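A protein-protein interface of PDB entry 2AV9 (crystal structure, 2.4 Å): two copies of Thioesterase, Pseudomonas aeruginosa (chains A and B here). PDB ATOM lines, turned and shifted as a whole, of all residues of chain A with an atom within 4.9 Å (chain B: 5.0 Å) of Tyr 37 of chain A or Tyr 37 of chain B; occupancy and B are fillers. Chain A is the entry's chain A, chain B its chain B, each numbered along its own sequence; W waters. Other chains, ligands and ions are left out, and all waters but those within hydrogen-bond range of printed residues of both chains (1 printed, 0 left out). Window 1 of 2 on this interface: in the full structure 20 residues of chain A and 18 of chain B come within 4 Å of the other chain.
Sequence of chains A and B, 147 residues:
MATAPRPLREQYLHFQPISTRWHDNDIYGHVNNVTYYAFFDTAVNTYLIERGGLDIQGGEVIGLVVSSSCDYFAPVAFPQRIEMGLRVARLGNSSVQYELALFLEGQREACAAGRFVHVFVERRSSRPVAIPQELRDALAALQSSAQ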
ATOM      1  N   ASN A  33     -13.002 -17.807  -9.327  1.00  0.00           N
ATOM      2  CA  ASN A  33     -14.428 -18.044  -9.468  1.00  0.00           C
ATOM      3  C   ASN A  33     -14.910 -18.244 -10.899  1.00  0.00           C
ATOM      4  O   ASN A  33     -15.857 -18.992 -11.135  1.00  0.00           O
ATOM      5  CB  ASN A  33     -15.219 -16.906  -8.814  1.00  0.00           C
ATOM      6  CG  ASN A  33     -14.667 -15.528  -9.157  1.00  0.00           C
ATOM      7  OD1 ASN A  33     -13.638 -15.113  -8.621  1.00  0.00           O
ATOM      8  ND2 ASN A  33     -15.362 -14.790 -10.025  1.00  0.00           N
ATOM      9  N   VAL A  34     -14.266 -17.572 -11.845  1.00  0.00           N
ATOM     10  CA  VAL A  34     -14.619 -17.650 -13.259  1.00  0.00           C
ATOM     11  C   VAL A  34     -14.378 -19.049 -13.846  1.00  0.00           C
ATOM     12  O   VAL A  34     -15.177 -19.506 -14.666  1.00  0.00           O
ATOM     13  CB  VAL A  34     -13.881 -16.527 -14.013  1.00  0.00           C
ATOM     14  CG1 VAL A  34     -13.934 -16.779 -15.490  1.00  0.00           C
ATOM     15  CG2 VAL A  34     -14.445 -15.172 -13.633  1.00  0.00           C
ATOM     16  N   THR A  35     -13.326 -19.722 -13.382  1.00  0.00           N
ATOM     17  CA  THR A  35     -12.901 -21.031 -13.877  1.00  0.00           C
ATOM     18  C   THR A  35     -13.986 -22.080 -13.608  1.00  0.00           C
ATOM     19  O   THR A  35     -14.169 -23.028 -14.364  1.00  0.00           O
ATOM     20  CB  THR A  35     -11.498 -21.378 -13.280  1.00  0.00           C
ATOM     21  OG1 THR A  35     -10.576 -20.300 -13.519  1.00  0.00           O
ATOM     22  CG2 THR A  35     -10.898 -22.622 -13.915  1.00  0.00           C
ATOM     23  N   TYR A  36     -14.791 -21.885 -12.574  1.00  0.00           N
ATOM     24  CA  TYR A  36     -15.822 -22.866 -12.253  1.00  0.00           C
ATOM     25  C   TYR A  36     -16.790 -23.082 -13.411  1.00  0.00           C
ATOM     26  O   TYR A  36     -17.322 -24.163 -13.662  1.00  0.00           O
ATOM     27  CB  TYR A  36     -16.547 -22.451 -10.961  1.00  0.00           C
ATOM     28  CG  TYR A  36     -15.742 -22.687  -9.680  1.00  0.00           C
ATOM     29  CD1 TYR A  36     -14.658 -21.876  -9.338  1.00  0.00           C
ATOM     30  CD2 TYR A  36     -16.062 -23.715  -8.797  1.00  0.00           C
ATOM     31  CE1 TYR A  36     -13.909 -22.075  -8.184  1.00  0.00           C
ATOM     32  CE2 TYR A  36     -15.325 -23.934  -7.621  1.00  0.00           C
ATOM     33  CZ  TYR A  36     -14.257 -23.101  -7.325  1.00  0.00           C
ATOM     34  OH  TYR A  36     -13.536 -23.270  -6.162  1.00  0.00           O
ATOM     35  N   TYR A  37     -17.014 -22.021 -14.174  1.00  0.00           N
ATOM     36  CA  TYR A  37     -17.932 -22.081 -15.301  1.00  0.00           C
ATOM     37  C   TYR A  37     -17.312 -22.782 -16.494  1.00  0.00           C
ATOM     38  O   TYR A  37     -18.046 -23.306 -17.335  1.00  0.00           O
ATOM     39  CB  TYR A  37     -18.315 -20.650 -15.695  1.00  0.00           C
ATOM     40  CG  TYR A  37     -19.227 -19.995 -14.678  1.00  0.00           C
ATOM     41  CD1 TYR A  37     -18.729 -19.042 -13.777  1.00  0.00           C
ATOM     42  CD2 TYR A  37     -20.575 -20.363 -14.601  1.00  0.00           C
ATOM     43  CE1 TYR A  37     -19.570 -18.448 -12.838  1.00  0.00           C
ATOM     44  CE2 TYR A  37     -21.417 -19.771 -13.684  1.00  0.00           C
ATOM     45  CZ  TYR A  37     -20.910 -18.798 -12.833  1.00  0.00           C
ATOM     46  OH  TYR A  37     -21.758 -18.238 -11.908  1.00  0.00           O
ATOM     47  N   ALA A  38     -15.981 -22.787 -16.590  1.00  0.00           N
ATOM     48  CA  ALA A  38     -15.278 -23.619 -17.577  1.00  0.00           C
ATOM     49  C   ALA A  38     -15.408 -25.095 -17.197  1.00  0.00           C
ATOM     50  O   ALA A  38     -15.558 -25.948 -18.077  1.00  0.00           O
ATOM     51  CB  ALA A  38     -13.809 -23.208 -17.771  1.00  0.00           C
ATOM     52  N   PHE A  39     -15.398 -25.397 -15.902  1.00  0.00           N
ATOM     53  CA  PHE A  39     -15.683 -26.763 -15.439  1.00  0.00           C
ATOM     54  C   PHE A  39     -17.109 -27.158 -15.818  1.00  0.00           C
ATOM     55  O   PHE A  39     -17.343 -28.288 -16.249  1.00  0.00           O
ATOM     56  CB  PHE A  39     -15.498 -26.927 -13.916  1.00  0.00           C
ATOM     57  CG  PHE A  39     -14.108 -26.584 -13.435  1.00  0.00           C
ATOM     58  CD1 PHE A  39     -13.007 -26.739 -14.276  1.00  0.00           C
ATOM     59  CD2 PHE A  39     -13.891 -26.124 -12.140  1.00  0.00           C
ATOM     60  CE1 PHE A  39     -11.710 -26.453 -13.820  1.00  0.00           C
ATOM     61  CE2 PHE A  39     -12.619 -25.791 -11.675  1.00  0.00           C
ATOM     62  CZ  PHE A  39     -11.518 -25.969 -12.526  1.00  0.00           C
ATOM     63  N   PHE A  40     -18.068 -26.249 -15.640  1.00  0.00           N
ATOM     64  CA  PHE A  40     -19.471 -26.537 -15.996  1.00  0.00           C
ATOM     65  C   PHE A  40     -19.573 -26.876 -17.481  1.00  0.00           C
ATOM     66  O   PHE A  40     -20.120 -27.907 -17.891  1.00  0.00           O
ATOM     67  CB  PHE A  40     -20.385 -25.311 -15.848  1.00  0.00           C
ATOM     68  CG  PHE A  40     -20.715 -24.982 -14.422  1.00  0.00           C
ATOM     69  CD1 PHE A  40     -20.082 -25.649 -13.395  1.00  0.00           C
ATOM     70  CD2 PHE A  40     -21.662 -24.027 -14.111  1.00  0.00           C
ATOM     71  CE1 PHE A  40     -20.394 -25.377 -12.081  1.00  0.00           C
ATOM     72  CE2 PHE A  40     -21.963 -23.740 -12.789  1.00  0.00           C
ATOM     73  CZ  PHE A  40     -21.331 -24.405 -11.774  1.00  0.00           C
ATOM     74  N   ASP A  41     -19.027 -25.963 -18.281  1.00  0.00           N
ATOM     75  CA  ASP A  41     -18.971 -26.136 -19.736  1.00  0.00           C
ATOM     76  C   ASP A  41     -18.305 -27.447 -20.155  1.00  0.00           C
ATOM     77  O   ASP A  41     -18.773 -28.133 -21.071  1.00  0.00           O
ATOM     78  CB  ASP A  41     -18.100 -25.042 -20.360  1.00  0.00           C
ATOM     79  CG  ASP A  41     -18.885 -23.950 -21.064  1.00  0.00           C
ATOM     80  OD1 ASP A  41     -20.115 -24.095 -21.243  1.00  0.00           O
ATOM     81  OD2 ASP A  41     -18.247 -22.945 -21.444  1.00  0.00           O
ATOM     82  N   SER A  68     -26.656 -18.963 -16.350  1.00  0.00           N
ATOM     83  CA  SER A  68     -25.838 -19.815 -15.505  1.00  0.00           C
ATOM     84  C   SER A  68     -25.655 -19.117 -14.165  1.00  0.00           C
ATOM     85  O   SER A  68     -25.815 -17.904 -14.067  1.00  0.00           O
ATOM     86  CB  SER A  68     -24.495 -20.086 -16.200  1.00  0.00           C
ATOM     87  OG  SER A  68     -23.758 -18.872 -16.211  1.00  0.00           O
ATOM     88  N   SER A  69     -25.315 -19.874 -13.128  1.00  0.00           N
ATOM     89  CA  SER A  69     -25.123 -19.263 -11.823  1.00  0.00           C
ATOM     90  C   SER A  69     -24.289 -20.208 -10.991  1.00  0.00           C
ATOM     91  O   SER A  69     -24.216 -21.412 -11.270  1.00  0.00           O
ATOM     92  CB  SER A  69     -26.462 -18.968 -11.138  1.00  0.00           C
ATOM     93  OG  SER A  69     -27.232 -20.148 -11.009  1.00  0.00           O
ATOM     94  N   CYS A  70     -23.632 -19.655  -9.979  1.00  0.00           N
ATOM     95  CA  CYS A  70     -22.814 -20.511  -9.115  1.00  0.00           C
ATOM     96  C   CYS A  70     -22.721 -19.913  -7.710  1.00  0.00           C
ATOM     97  O   CYS A  70     -22.656 -18.695  -7.533  1.00  0.00           O
ATOM     98  CB  CYS A  70     -21.453 -20.738  -9.776  1.00  0.00           C
ATOM     99  SG  CYS A  70     -20.355 -21.929  -8.941  1.00  0.00           S
ATOM    100  N   TYR A  72     -20.344 -20.373  -4.162  1.00  0.00           N
ATOM    101  CA  TYR A  72     -19.032 -20.894  -3.810  1.00  0.00           C
ATOM    102  C   TYR A  72     -18.909 -21.046  -2.298  1.00  0.00           C
ATOM    103  O   TYR A  72     -19.076 -20.060  -1.590  1.00  0.00           O
ATOM    104  CB  TYR A  72     -17.915 -19.979  -4.312  1.00  0.00           C
ATOM    105  CG  TYR A  72     -18.015 -19.601  -5.777  1.00  0.00           C
ATOM    106  CD1 TYR A  72     -18.890 -18.602  -6.217  1.00  0.00           C
ATOM    107  CD2 TYR A  72     -17.191 -20.201  -6.714  1.00  0.00           C
ATOM    108  CE1 TYR A  72     -18.971 -18.235  -7.563  1.00  0.00           C
ATOM    109  CE2 TYR A  72     -17.285 -19.857  -8.055  1.00  0.00           C
ATOM    110  CZ  TYR A  72     -18.152 -18.868  -8.470  1.00  0.00           C
ATOM    111  OH  TYR A  72     -18.200 -18.554  -9.812  1.00  0.00           O
ATOM    112  N   ASN B  33     -18.958 -18.296 -22.780  1.00  0.00           N
ATOM    113  CA  ASN B  33     -19.877 -17.708 -21.816  1.00  0.00           C
ATOM    114  C   ASN B  33     -19.115 -17.515 -20.518  1.00  0.00           C
ATOM    115  O   ASN B  33     -19.539 -16.812 -19.599  1.00  0.00           O
ATOM    116  CB  ASN B  33     -21.120 -18.572 -21.613  1.00  0.00           C
ATOM    117  CG  ASN B  33     -20.968 -19.919 -22.257  1.00  0.00           C
ATOM    118  OD1 ASN B  33     -20.532 -20.884 -21.622  1.00  0.00           O
ATOM    119  ND2 ASN B  33     -21.259 -19.959 -23.564  1.00  0.00           N
ATOM    120  N   VAL B  34     -17.966 -18.168 -20.422  1.00  0.00           N
ATOM    121  CA  VAL B  34     -17.144 -17.965 -19.247  1.00  0.00           C
ATOM    122  C   VAL B  34     -16.479 -16.598 -19.306  1.00  0.00           C
ATOM    123  O   VAL B  34     -16.353 -15.939 -18.278  1.00  0.00           O
ATOM    124  CB  VAL B  34     -16.085 -19.069 -19.136  1.00  0.00           C
ATOM    125  CG1 VAL B  34     -14.957 -18.749 -18.148  1.00  0.00           C
ATOM    126  CG2 VAL B  34     -16.776 -20.414 -18.857  1.00  0.00           C
ATOM    127  N   THR B  35     -16.048 -16.112 -20.468  1.00  0.00           N
ATOM    128  CA  THR B  35     -15.435 -14.797 -20.543  1.00  0.00           C
ATOM    129  C   THR B  35     -16.295 -13.659 -19.991  1.00  0.00           C
ATOM    130  O   THR B  35     -15.777 -12.640 -19.518  1.00  0.00           O
ATOM    131  CB  THR B  35     -15.139 -14.442 -22.017  1.00  0.00           C
ATOM    132  OG1 THR B  35     -14.344 -15.465 -22.641  1.00  0.00           O
ATOM    133  CG2 THR B  35     -14.407 -13.096 -22.169  1.00  0.00           C
ATOM    134  N   TYR B  36     -17.617 -13.771 -20.065  1.00  0.00           N
ATOM    135  CA  TYR B  36     -18.469 -12.742 -19.467  1.00  0.00           C
ATOM    136  C   TYR B  36     -18.238 -12.520 -17.974  1.00  0.00           C
ATOM    137  O   TYR B  36     -18.280 -11.381 -17.507  1.00  0.00           O
ATOM    138  CB  TYR B  36     -19.965 -13.045 -19.640  1.00  0.00           C
ATOM    139  CG  TYR B  36     -20.411 -13.005 -21.084  1.00  0.00           C
ATOM    140  CD1 TYR B  36     -19.884 -13.878 -22.041  1.00  0.00           C
ATOM    141  CD2 TYR B  36     -21.416 -12.132 -21.485  1.00  0.00           C
ATOM    142  CE1 TYR B  36     -20.328 -13.811 -23.363  1.00  0.00           C
ATOM    143  CE2 TYR B  36     -21.815 -12.044 -22.822  1.00  0.00           C
ATOM    144  CZ  TYR B  36     -21.304 -12.903 -23.760  1.00  0.00           C
ATOM    145  OH  TYR B  36     -21.799 -12.818 -25.053  1.00  0.00           O
ATOM    146  N   TYR B  37     -17.997 -13.589 -17.221  1.00  0.00           N
ATOM    147  CA  TYR B  37     -17.645 -13.407 -15.805  1.00  0.00           C
ATOM    148  C   TYR B  37     -16.306 -12.729 -15.574  1.00  0.00           C
ATOM    149  O   TYR B  37     -16.165 -12.051 -14.553  1.00  0.00           O
ATOM    150  CB  TYR B  37     -17.698 -14.732 -15.047  1.00  0.00           C
ATOM    151  CG  TYR B  37     -19.113 -15.298 -14.946  1.00  0.00           C
ATOM    152  CD1 TYR B  37     -19.562 -16.264 -15.838  1.00  0.00           C
ATOM    153  CD2 TYR B  37     -20.003 -14.851 -13.963  1.00  0.00           C
ATOM    154  CE1 TYR B  37     -20.847 -16.810 -15.731  1.00  0.00           C
ATOM    155  CE2 TYR B  37     -21.280 -15.368 -13.831  1.00  0.00           C
ATOM    156  CZ  TYR B  37     -21.676 -16.358 -14.709  1.00  0.00           C
ATOM    157  OH  TYR B  37     -22.939 -16.863 -14.564  1.00  0.00           O
ATOM    158  N   ALA B  38     -15.381 -12.910 -16.519  1.00  0.00           N
ATOM    159  CA  ALA B  38     -14.048 -12.306 -16.526  1.00  0.00           C
ATOM    160  C   ALA B  38     -14.231 -10.812 -16.713  1.00  0.00           C
ATOM    161  O   ALA B  38     -13.554 -10.014 -16.055  1.00  0.00           O
ATOM    162  CB  ALA B  38     -13.170 -12.885 -17.639  1.00  0.00           C
ATOM    163  N   PHE B  39     -15.173 -10.417 -17.564  1.00  0.00           N
ATOM    164  CA  PHE B  39     -15.524  -9.006 -17.729  1.00  0.00           C
ATOM    165  C   PHE B  39     -16.102  -8.414 -16.457  1.00  0.00           C
ATOM    166  O   PHE B  39     -15.697  -7.318 -16.064  1.00  0.00           O
ATOM    167  CB  PHE B  39     -16.522  -8.807 -18.871  1.00  0.00           C
ATOM    168  CG  PHE B  39     -15.902  -8.976 -20.218  1.00  0.00           C
ATOM    169  CD1 PHE B  39     -14.540  -9.253 -20.319  1.00  0.00           C
ATOM    170  CD2 PHE B  39     -16.660  -8.905 -21.368  1.00  0.00           C
ATOM    171  CE1 PHE B  39     -13.950  -9.423 -21.563  1.00  0.00           C
ATOM    172  CE2 PHE B  39     -16.063  -9.069 -22.634  1.00  0.00           C
ATOM    173  CZ  PHE B  39     -14.715  -9.330 -22.723  1.00  0.00           C
ATOM    174  N   PHE B  40     -17.060  -9.109 -15.851  1.00  0.00           N
ATOM    175  CA  PHE B  40     -17.629  -8.645 -14.583  1.00  0.00           C
ATOM    176  C   PHE B  40     -16.525  -8.352 -13.560  1.00  0.00           C
ATOM    177  O   PHE B  40     -16.515  -7.281 -12.974  1.00  0.00           O
ATOM    178  CB  PHE B  40     -18.589  -9.661 -13.947  1.00  0.00           C
ATOM    179  CG  PHE B  40     -19.817  -9.939 -14.750  1.00  0.00           C
ATOM    180  CD1 PHE B  40     -20.200  -9.093 -15.761  1.00  0.00           C
ATOM    181  CD2 PHE B  40     -20.625 -11.020 -14.435  1.00  0.00           C
ATOM    182  CE1 PHE B  40     -21.334  -9.340 -16.518  1.00  0.00           C
ATOM    183  CE2 PHE B  40     -21.765 -11.288 -15.176  1.00  0.00           C
ATOM    184  CZ  PHE B  40     -22.130 -10.428 -16.209  1.00  0.00           C
ATOM    185  N   ASP B  41     -15.609  -9.295 -13.361  1.00  0.00           N
ATOM    186  CA  ASP B  41     -14.514  -9.153 -12.421  1.00  0.00           C
ATOM    187  C   ASP B  41     -13.548  -8.060 -12.828  1.00  0.00           C
ATOM    188  O   ASP B  41     -13.033  -7.382 -11.936  1.00  0.00           O
ATOM    189  CB  ASP B  41     -13.729 -10.462 -12.265  1.00  0.00           C
ATOM    190  CG  ASP B  41     -14.522 -11.506 -11.508  1.00  0.00           C
ATOM    191  OD1 ASP B  41     -15.655 -11.209 -11.049  1.00  0.00           O
ATOM    192  OD2 ASP B  41     -14.006 -12.635 -11.388  1.00  0.00           O
ATOM    193  N   SER B  68     -22.409 -15.693  -8.091  1.00  0.00           N
ATOM    194  CA  SER B  68     -22.461 -14.977  -9.365  1.00  0.00           C
ATOM    195  C   SER B  68     -23.486 -15.635 -10.282  1.00  0.00           C
ATOM    196  O   SER B  68     -23.791 -16.814 -10.169  1.00  0.00           O
ATOM    197  CB  SER B  68     -21.100 -14.987 -10.080  1.00  0.00           C
ATOM    198  OG  SER B  68     -20.632 -16.321 -10.198  1.00  0.00           O
ATOM    199  N   SER B  69     -24.015 -14.861 -11.219  1.00  0.00           N
ATOM    200  CA  SER B  69     -24.879 -15.424 -12.255  1.00  0.00           C
ATOM    201  C   SER B  69     -24.911 -14.497 -13.466  1.00  0.00           C
ATOM    202  O   SER B  69     -24.429 -13.350 -13.411  1.00  0.00           O
ATOM    203  CB  SER B  69     -26.293 -15.661 -11.725  1.00  0.00           C
ATOM    204  OG  SER B  69     -26.901 -14.471 -11.272  1.00  0.00           O
ATOM    205  N   CYS B  70     -25.436 -15.037 -14.563  1.00  0.00           N
ATOM    206  CA  CYS B  70     -25.445 -14.343 -15.834  1.00  0.00           C
ATOM    207  C   CYS B  70     -26.551 -14.842 -16.751  1.00  0.00           C
ATOM    208  O   CYS B  70     -26.731 -16.051 -16.858  1.00  0.00           O
ATOM    209  CB  CYS B  70     -24.105 -14.548 -16.541  1.00  0.00           C
ATOM    210  SG  CYS B  70     -23.849 -13.406 -17.928  1.00  0.00           S
ATOM    211  N   TYR B  72     -27.829 -14.563 -20.835  1.00  0.00           N
ATOM    212  CA  TYR B  72     -27.162 -14.237 -22.106  1.00  0.00           C
ATOM    213  C   TYR B  72     -28.266 -14.053 -23.135  1.00  0.00           C
ATOM    214  O   TYR B  72     -29.091 -14.943 -23.334  1.00  0.00           O
ATOM    215  CB  TYR B  72     -26.170 -15.296 -22.626  1.00  0.00           C
ATOM    216  CG  TYR B  72     -25.100 -15.759 -21.638  1.00  0.00           C
ATOM    217  CD1 TYR B  72     -25.386 -16.625 -20.573  1.00  0.00           C
ATOM    218  CD2 TYR B  72     -23.796 -15.314 -21.747  1.00  0.00           C
ATOM    219  CE1 TYR B  72     -24.407 -17.036 -19.677  1.00  0.00           C
ATOM    220  CE2 TYR B  72     -22.811 -15.715 -20.858  1.00  0.00           C
ATOM    221  CZ  TYR B  72     -23.096 -16.581 -19.824  1.00  0.00           C
ATOM    222  OH  TYR B  72     -22.054 -16.934 -18.980  1.00  0.00           O
HETATM  223  O   HOH W   1     -21.790 -19.508 -18.084  1.00  0.00           O
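Among the printed residues, pairs that only touch across the chains: Ser 68 of chain A with Ser 69 of chain B (3.2 Å), Ser 69 of chain A with Ser 68 of chain B (3.2 Å), Ser 69 of chain A with Ser 69 of chain B (3.4 Å), Ala 38 of chain A with Val 34 of chain B (3.4 Å), Tyr 37 of chain A with Val 34 of chain B (3.4 Å), Val 34 of chain A with Asp 41 of chain B (3.4 Å), Val 34 of chain A with Val 34 of chain B (3.5 Å), Val 34 of chain A with Tyr 37 of chain B (3.6 Å), Val 34 of chain A with Ala 38 of chain B (3.8 Å), Ser 68 of chain A with Tyr 72 of chain B (3.8 Å) and Asp 41 of chain A with Val 34 of chain B (3.9 Å).
Asn 33 of chain A touches Asp 41 of chain B, and with the chains exchanged Asp 41 of chain A touches Asn 33 of chain B. Val 34 of chain A touches Ala 38 of chain B, and with the chains exchanged Ala 38 of chain A touches Val 34 of chain B. Val 34 of chain A touches Asp 41 of chain B, and with the chains exchanged Asp 41 of chain A touches Val 34 of chain B. Ser 68 of chain A touches Ser 69 of chain B, and with the chains exchanged Ser 69 of chain A touches Ser 68 of chain B. Of the 19 pairs that touch across the chains among the printed residues, 19 have their exchanged pair printed and touching as well.
Of chain B, only Val 34, Tyr 37 and Ser 68 come within 4 Å of Tyr 37 of chain A. Of chain A, only Val 34 (3.6 Å), Tyr 37 (3.2 Å) and Ser 68 (2.7 Å) come within 4 Å of Tyr 37 of chain B. Printed residues of chain B within 4 Å of Ala 38 of chain A: Val 34. Of the printed residues of chain A, Tyr 72 of chain B touches Ser 68. Of the printed residues of chain B, Asp 41 of chain A touches Asn 33 (3.1 Å) and Val 34 (3.9 Å). Of the printed residues of chain A, Asn 33 of chain B touches Asp 41. The nearest residue of chain B that does not touch Tyr 37 of chain A is Ser 69 of chain B (4.1 Å).
The side-chain carboxylate (OD2) of Asp 41 of chain A sits close to the side-chain amide oxygen (OD1) of Asn 33 of chain B (3.1 Å). The side-chain hydroxyl of Ser 68 of chain B lies within hydrogen-bond range of the side-chain hydroxyl of Tyr 72 of chain A, at 3.3 Å. OD2 of Asp 41 of chain B is in hydrogen-bond range of ND2 of Asn 33 of chain A (2.9 Å). The backbone carbonyl oxygen (O) of Ser 68 of chain A is in hydrogen-bond range of the backbone NH (N) of Cys 70 of chain B, 2.9 Å away. OG of Ser 68 of chain B sits at hydrogen-bond distance from OH of Tyr 37 of chain A (2.8 Å). The side-chain hydroxyl (OH) of Tyr 37 of chain B sits at hydrogen-bond distance from the side-chain hydroxyl (OG) of Ser 68 of chain A (2.7 Å). N of Cys 70 of chain A sits at hydrogen-bond distance from O of Ser 68 of chain B, at 2.9 Å. OH of Tyr 37 of chain B sits at hydrogen-bond distance from OH of Tyr 37 of chain A (3.2 Å).
Of the 13 printed residues of chain B, 9 touch a printed residue of chain A. Hydrophobic or aromatic side chains of chain A within 4 Å of the printed part of chain B: Val 34, Tyr 37 and Tyr 72.
Water W1 lies within hydrogen-bond range of OH of Tyr 72 of chain B and OG of Ser 68 of chain A.
OH of Tyr 37 of chain A sits at hydrogen-bond distance from N of Cys 70 of chain A, at 3.0 Å. The backbone NH of Cys 70 of chain B sits at hydrogen-bond distance from the side-chain hydroxyl of Tyr 37 of chain B. O of Asn 33 of chain B is in hydrogen-bond range of OH of Tyr 72 of chain B, at 2.6 Å. The backbone carbonyl oxygen (O) of Asn 33 of chain A lies within hydrogen-bond range of the side-chain hydroxyl (OH) of Tyr 72 of chain A (2.7 Å).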
